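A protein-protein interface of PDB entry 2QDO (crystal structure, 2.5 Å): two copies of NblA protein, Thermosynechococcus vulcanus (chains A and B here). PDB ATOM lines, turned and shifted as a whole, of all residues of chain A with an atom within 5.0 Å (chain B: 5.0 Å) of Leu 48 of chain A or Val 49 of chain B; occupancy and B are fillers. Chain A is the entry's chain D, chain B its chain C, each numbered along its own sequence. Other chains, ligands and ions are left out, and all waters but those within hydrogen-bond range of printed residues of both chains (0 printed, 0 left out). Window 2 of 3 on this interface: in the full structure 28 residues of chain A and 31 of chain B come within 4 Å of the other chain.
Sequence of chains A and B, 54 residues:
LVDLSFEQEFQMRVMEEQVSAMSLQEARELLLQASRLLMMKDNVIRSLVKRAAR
CG1 of Ile 45 of chain B touches CD1 of Ile 45 of chain A (3.2 Å).
CD2 of Leu 48 of chain B touches CD1 of Ile 45 of chain A (3.7 Å).
Leu 48 of chain B touches Leu 48 of chain A (CD2 to CB, 3.8 Å).
Val 49 of chain B touches Leu 48 of chain A (CG2 to CD2, 3.9 Å).
Hydrophobic or aromatic side chains of chain A that line the printed part of chain B: Ile 45 and Leu 48.
Among the printed residues, no Asp or Glu carboxylate lies within 4 Å of a Lys or Arg side-chain nitrogen of the other chain.
Ile 45 of chain A touches its own counterpart, Ile 45 of chain B.
Ile 45 of chain A touches Leu 48 of chain B, but with the chains exchanged Leu 48 of chain A does not touch Ile 45 of chain B (4.1 Å).
Leu 48 of chain A touches its own counterpart, Leu 48 of chain B.
Leu 48 of chain A touches Val 49 of chain B, but with the chains exchanged Val 49 of chain A does not touch Leu 48 of chain B (4.02 Å).
Positions printed for both chains: 45, 46, 47, 48, 49, 50 and 51.
Of the 4 pairs that touch across the chains among the printed residues, 2 have their exchanged pair printed and touching as well.
Of chain B, only Leu 48 (3.8 Å) and Val 49 (3.9 Å) come within 4 Å of Leu 48 of chain A.
Of chain A, only Leu 48 (3.9 Å) comes within 4 Å of Val 49 of chain B.
Of the printed residues of chain A, Leu 48 of chain B touches Ile 45 and Leu 48.
Printed residues of chain A within 4 Å of Ile 45 of chain B: Ile 45 (3.2 Å).
Printed residues of chain B within 4 Å of Ile 45 of chain A: Ile 45 (3.2 Å) and Leu 48 (3.7 Å).
Ala 53 of chain B touches none of the printed residues of chain A.
Arg 46 of chain A touches none of the printed residues of chain B.
The nearest residue of chain B that does not touch Leu 48 of chain A is Ile 45 of chain B (4.1 Å).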
ATOM      1  N   VAL A  44     -22.082 -23.741 -16.199  1.00  0.00           N
ATOM      2  CA  VAL A  44     -20.740 -23.240 -16.421  1.00  0.00           C
ATOM      3  C   VAL A  44     -19.743 -24.383 -16.379  1.00  0.00           C
ATOM      4  O   VAL A  44     -18.830 -24.443 -17.197  1.00  0.00           O
ATOM      5  CB  VAL A  44     -20.331 -22.208 -15.362  1.00  0.00           C
ATOM      6  CG1 VAL A  44     -18.834 -21.820 -15.532  1.00  0.00           C
ATOM      7  CG2 VAL A  44     -21.210 -20.997 -15.472  1.00  0.00           C
ATOM      8  N   ILE A  45     -19.920 -25.283 -15.421  1.00  0.00           N
ATOM      9  CA  ILE A  45     -19.013 -26.411 -15.267  1.00  0.00           C
ATOM     10  C   ILE A  45     -19.054 -27.332 -16.465  1.00  0.00           C
ATOM     11  O   ILE A  45     -18.025 -27.869 -16.885  1.00  0.00           O
ATOM     12  CB  ILE A  45     -19.344 -27.222 -13.988  1.00  0.00           C
ATOM     13  CG1 ILE A  45     -18.869 -26.446 -12.763  1.00  0.00           C
ATOM     14  CG2 ILE A  45     -18.671 -28.581 -14.023  1.00  0.00           C
ATOM     15  CD1 ILE A  45     -17.330 -26.333 -12.560  1.00  0.00           C
ATOM     16  N   ARG A  46     -20.260 -27.515 -16.990  1.00  0.00           N
ATOM     17  CA  ARG A  46     -20.524 -28.368 -18.141  1.00  0.00           C
ATOM     18  C   ARG A  46     -19.825 -27.767 -19.366  1.00  0.00           C
ATOM     19  O   ARG A  46     -19.253 -28.494 -20.180  1.00  0.00           O
ATOM     20  CB  ARG A  46     -22.049 -28.472 -18.324  1.00  0.00           C
ATOM     21  CG  ARG A  46     -22.560 -29.399 -19.411  1.00  0.00           C
ATOM     22  CD  ARG A  46     -24.082 -29.603 -19.287  1.00  0.00           C
ATOM     23  NE  ARG A  46     -24.446 -30.189 -17.996  1.00  0.00           N
ATOM     24  CZ  ARG A  46     -25.120 -29.557 -17.034  1.00  0.00           C
ATOM     25  NH1 ARG A  46     -25.396 -30.183 -15.894  1.00  0.00           N
ATOM     26  NH2 ARG A  46     -25.536 -28.308 -17.206  1.00  0.00           N
ATOM     27  N   SER A  47     -19.869 -26.441 -19.480  1.00  0.00           N
ATOM     28  CA  SER A  47     -19.203 -25.735 -20.569  1.00  0.00           C
ATOM     29  C   SER A  47     -17.720 -26.075 -20.540  1.00  0.00           C
ATOM     30  O   SER A  47     -17.192 -26.733 -21.443  1.00  0.00           O
ATOM     31  CB  SER A  47     -19.336 -24.223 -20.398  1.00  0.00           C
ATOM     32  OG  SER A  47     -20.524 -23.723 -20.970  1.00  0.00           O
ATOM     33  N   LEU A  48     -17.055 -25.595 -19.497  1.00  0.00           N
ATOM     34  CA  LEU A  48     -15.635 -25.820 -19.312  1.00  0.00           C
ATOM     35  C   LEU A  48     -15.239 -27.274 -19.459  1.00  0.00           C
ATOM     36  O   LEU A  48     -14.110 -27.573 -19.846  1.00  0.00           O
ATOM     37  CB  LEU A  48     -15.192 -25.302 -17.947  1.00  0.00           C
ATOM     38  CG  LEU A  48     -14.976 -23.792 -17.791  1.00  0.00           C
ATOM     39  CD1 LEU A  48     -15.740 -22.990 -18.828  1.00  0.00           C
ATOM     40  CD2 LEU A  48     -15.389 -23.402 -16.386  1.00  0.00           C
ATOM     41  N   VAL A  49     -16.143 -28.192 -19.157  1.00  0.00           N
ATOM     42  CA  VAL A  49     -15.767 -29.582 -19.330  1.00  0.00           C
ATOM     43  C   VAL A  49     -15.876 -29.914 -20.812  1.00  0.00           C
ATOM     44  O   VAL A  49     -15.120 -30.746 -21.324  1.00  0.00           O
ATOM     45  CB  VAL A  49     -16.648 -30.552 -18.488  1.00  0.00           C
ATOM     46  CG1 VAL A  49     -16.508 -31.990 -18.997  1.00  0.00           C
ATOM     47  CG2 VAL A  49     -16.201 -30.505 -17.025  1.00  0.00           C
ATOM     48  N   LYS A  50     -16.791 -29.245 -21.515  1.00  0.00           N
ATOM     49  CA  LYS A  50     -16.950 -29.533 -22.934  1.00  0.00           C
ATOM     50  C   LYS A  50     -15.713 -29.173 -23.762  1.00  0.00           C
ATOM     51  O   LYS A  50     -15.483 -29.797 -24.794  1.00  0.00           O
ATOM     52  CB  LYS A  50     -18.209 -28.881 -23.510  1.00  0.00           C
ATOM     53  CG  LYS A  50     -18.600 -29.452 -24.872  1.00  0.00           C
ATOM     54  CD  LYS A  50     -20.112 -29.481 -25.070  1.00  0.00           C
ATOM     55  CE  LYS A  50     -20.511 -29.433 -26.543  1.00  0.00           C
ATOM     56  NZ  LYS A  50     -21.051 -28.090 -26.898  1.00  0.00           N
ATOM     57  N   ARG A  51     -14.925 -28.170 -23.361  1.00  0.00           N
ATOM     58  CA  ARG A  51     -13.681 -27.933 -24.100  1.00  0.00           C
ATOM     59  C   ARG A  51     -12.876 -29.159 -23.668  1.00  0.00           C
ATOM     60  O   ARG A  51     -11.853 -29.038 -22.988  1.00  0.00           O
ATOM     61  CB  ARG A  51     -12.958 -26.683 -23.644  1.00  0.00           C
ATOM     62  N   ILE B  45     -15.076 -24.841 -10.523  1.00  0.00           N
ATOM     63  CA  ILE B  45     -14.906 -23.915 -11.639  1.00  0.00           C
ATOM     64  C   ILE B  45     -13.494 -23.339 -11.622  1.00  0.00           C
ATOM     65  O   ILE B  45     -12.740 -23.512 -12.577  1.00  0.00           O
ATOM     66  CB  ILE B  45     -15.935 -22.745 -11.575  1.00  0.00           C
ATOM     67  CG1 ILE B  45     -17.363 -23.274 -11.758  1.00  0.00           C
ATOM     68  CG2 ILE B  45     -15.626 -21.726 -12.651  1.00  0.00           C
ATOM     69  CD1 ILE B  45     -18.469 -22.303 -11.345  1.00  0.00           C
ATOM     70  N   ARG B  46     -13.134 -22.658 -10.537  1.00  0.00           N
ATOM     71  CA  ARG B  46     -11.794 -22.086 -10.432  1.00  0.00           C
ATOM     72  C   ARG B  46     -10.740 -23.119 -10.849  1.00  0.00           C
ATOM     73  O   ARG B  46      -9.905 -22.854 -11.705  1.00  0.00           O
ATOM     74  CB  ARG B  46     -11.508 -21.620  -8.995  1.00  0.00           C
ATOM     75  CG  ARG B  46     -12.409 -20.504  -8.482  1.00  0.00           C
ATOM     76  CD  ARG B  46     -11.874 -19.884  -7.186  1.00  0.00           C
ATOM     77  NE  ARG B  46     -12.689 -18.760  -6.722  1.00  0.00           N
ATOM     78  CZ  ARG B  46     -13.586 -18.831  -5.740  1.00  0.00           C
ATOM     79  NH1 ARG B  46     -14.282 -17.755  -5.393  1.00  0.00           N
ATOM     80  NH2 ARG B  46     -13.777 -19.972  -5.091  1.00  0.00           N
ATOM     81  N   SER B  47     -10.797 -24.294 -10.234  1.00  0.00           N
ATOM     82  CA  SER B  47      -9.865 -25.387 -10.509  1.00  0.00           C
ATOM     83  C   SER B  47      -9.856 -25.886 -11.947  1.00  0.00           C
ATOM     84  O   SER B  47      -8.871 -26.471 -12.404  1.00  0.00           O
ATOM     85  CB  SER B  47     -10.183 -26.563  -9.589  1.00  0.00           C
ATOM     86  OG  SER B  47      -9.755 -27.790 -10.150  1.00  0.00           O
ATOM     87  N   LEU B  48     -10.961 -25.652 -12.643  1.00  0.00           N
ATOM     88  CA  LEU B  48     -11.159 -26.087 -14.018  1.00  0.00           C
ATOM     89  C   LEU B  48     -10.605 -25.054 -14.997  1.00  0.00           C
ATOM     90  O   LEU B  48     -10.125 -25.386 -16.089  1.00  0.00           O
ATOM     91  CB  LEU B  48     -12.658 -26.273 -14.240  1.00  0.00           C
ATOM     92  CG  LEU B  48     -13.211 -27.433 -15.058  1.00  0.00           C
ATOM     93  CD1 LEU B  48     -12.619 -28.753 -14.593  1.00  0.00           C
ATOM     94  CD2 LEU B  48     -14.722 -27.438 -14.890  1.00  0.00           C
ATOM     95  N   VAL B  49     -10.702 -23.797 -14.590  1.00  0.00           N
ATOM     96  CA  VAL B  49     -10.218 -22.675 -15.368  1.00  0.00           C
ATOM     97  C   VAL B  49      -8.695 -22.610 -15.273  1.00  0.00           C
ATOM     98  O   VAL B  49      -8.017 -22.249 -16.238  1.00  0.00           O
ATOM     99  CB  VAL B  49     -10.861 -21.364 -14.858  1.00  0.00           C
ATOM    100  CG1 VAL B  49     -10.035 -20.148 -15.268  1.00  0.00           C
ATOM    101  CG2 VAL B  49     -12.255 -21.245 -15.434  1.00  0.00           C
ATOM    102  N   LYS B  50      -8.151 -22.959 -14.111  1.00  0.00           N
ATOM    103  CA  LYS B  50      -6.705 -22.954 -13.962  1.00  0.00           C
ATOM    104  C   LYS B  50      -6.192 -24.094 -14.847  1.00  0.00           C
ATOM    105  O   LYS B  50      -5.400 -23.876 -15.761  1.00  0.00           O
ATOM    106  CB  LYS B  50      -6.303 -23.192 -12.498  1.00  0.00           C
ATOM    107  CG  LYS B  50      -6.996 -22.269 -11.485  1.00  0.00           C
ATOM    108  CD  LYS B  50      -6.060 -21.260 -10.814  1.00  0.00           C
ATOM    109  CE  LYS B  50      -6.249 -19.850 -11.367  1.00  0.00           C
ATOM    110  NZ  LYS B  50      -6.023 -18.791 -10.337  1.00  0.00           N
ATOM    111  N   ARG B  51      -6.686 -25.303 -14.588  1.00  0.00           N
ATOM    112  CA  ARG B  51      -6.286 -26.494 -15.334  1.00  0.00           C
ATOM    113  C   ARG B  51      -6.410 -26.369 -16.851  1.00  0.00           C
ATOM    114  O   ARG B  51      -5.837 -27.171 -17.581  1.00  0.00           O
ATOM    115  CB  ARG B  51      -7.084 -27.718 -14.861  1.00  0.00           C
ATOM    116  CG  ARG B  51      -6.704 -29.020 -15.566  1.00  0.00           C
ATOM    117  CD  ARG B  51      -7.426 -30.213 -14.965  1.00  0.00           C
ATOM    118  NE  ARG B  51      -6.778 -31.488 -15.269  1.00  0.00           N
ATOM    119  CZ  ARG B  51      -6.733 -32.054 -16.473  1.00  0.00           C
ATOM    120  NH1 ARG B  51      -7.303 -31.466 -17.518  1.00  0.00           N
ATOM    121  NH2 ARG B  51      -6.116 -33.218 -16.633  1.00  0.00           N
ATOM    122  N   ALA B  52      -7.170 -25.397 -17.338  1.00  0.00           N
ATOM    123  CA  ALA B  52      -7.288 -25.234 -18.781  1.00  0.00           C
ATOM    124  C   ALA B  52      -6.120 -24.356 -19.229  1.00  0.00           C
ATOM    125  O   ALA B  52      -5.372 -24.715 -20.140  1.00  0.00           O
ATOM    126  CB  ALA B  52      -8.619 -24.585 -19.146  1.00  0.00           C
ATOM    127  N   ALA B  53      -5.954 -23.215 -18.565  1.00  0.00           N
ATOM    128  CA  ALA B  53      -4.877 -22.283 -18.885  1.00  0.00           C
ATOM    129  C   ALA B  53      -3.528 -23.003 -18.918  1.00  0.00           C
ATOM    130  O   ALA B  53      -2.834 -22.978 -19.930  1.00  0.00           O
ATOM    131  CB  ALA B  53      -4.848 -21.150 -17.862  1.00  0.00           C
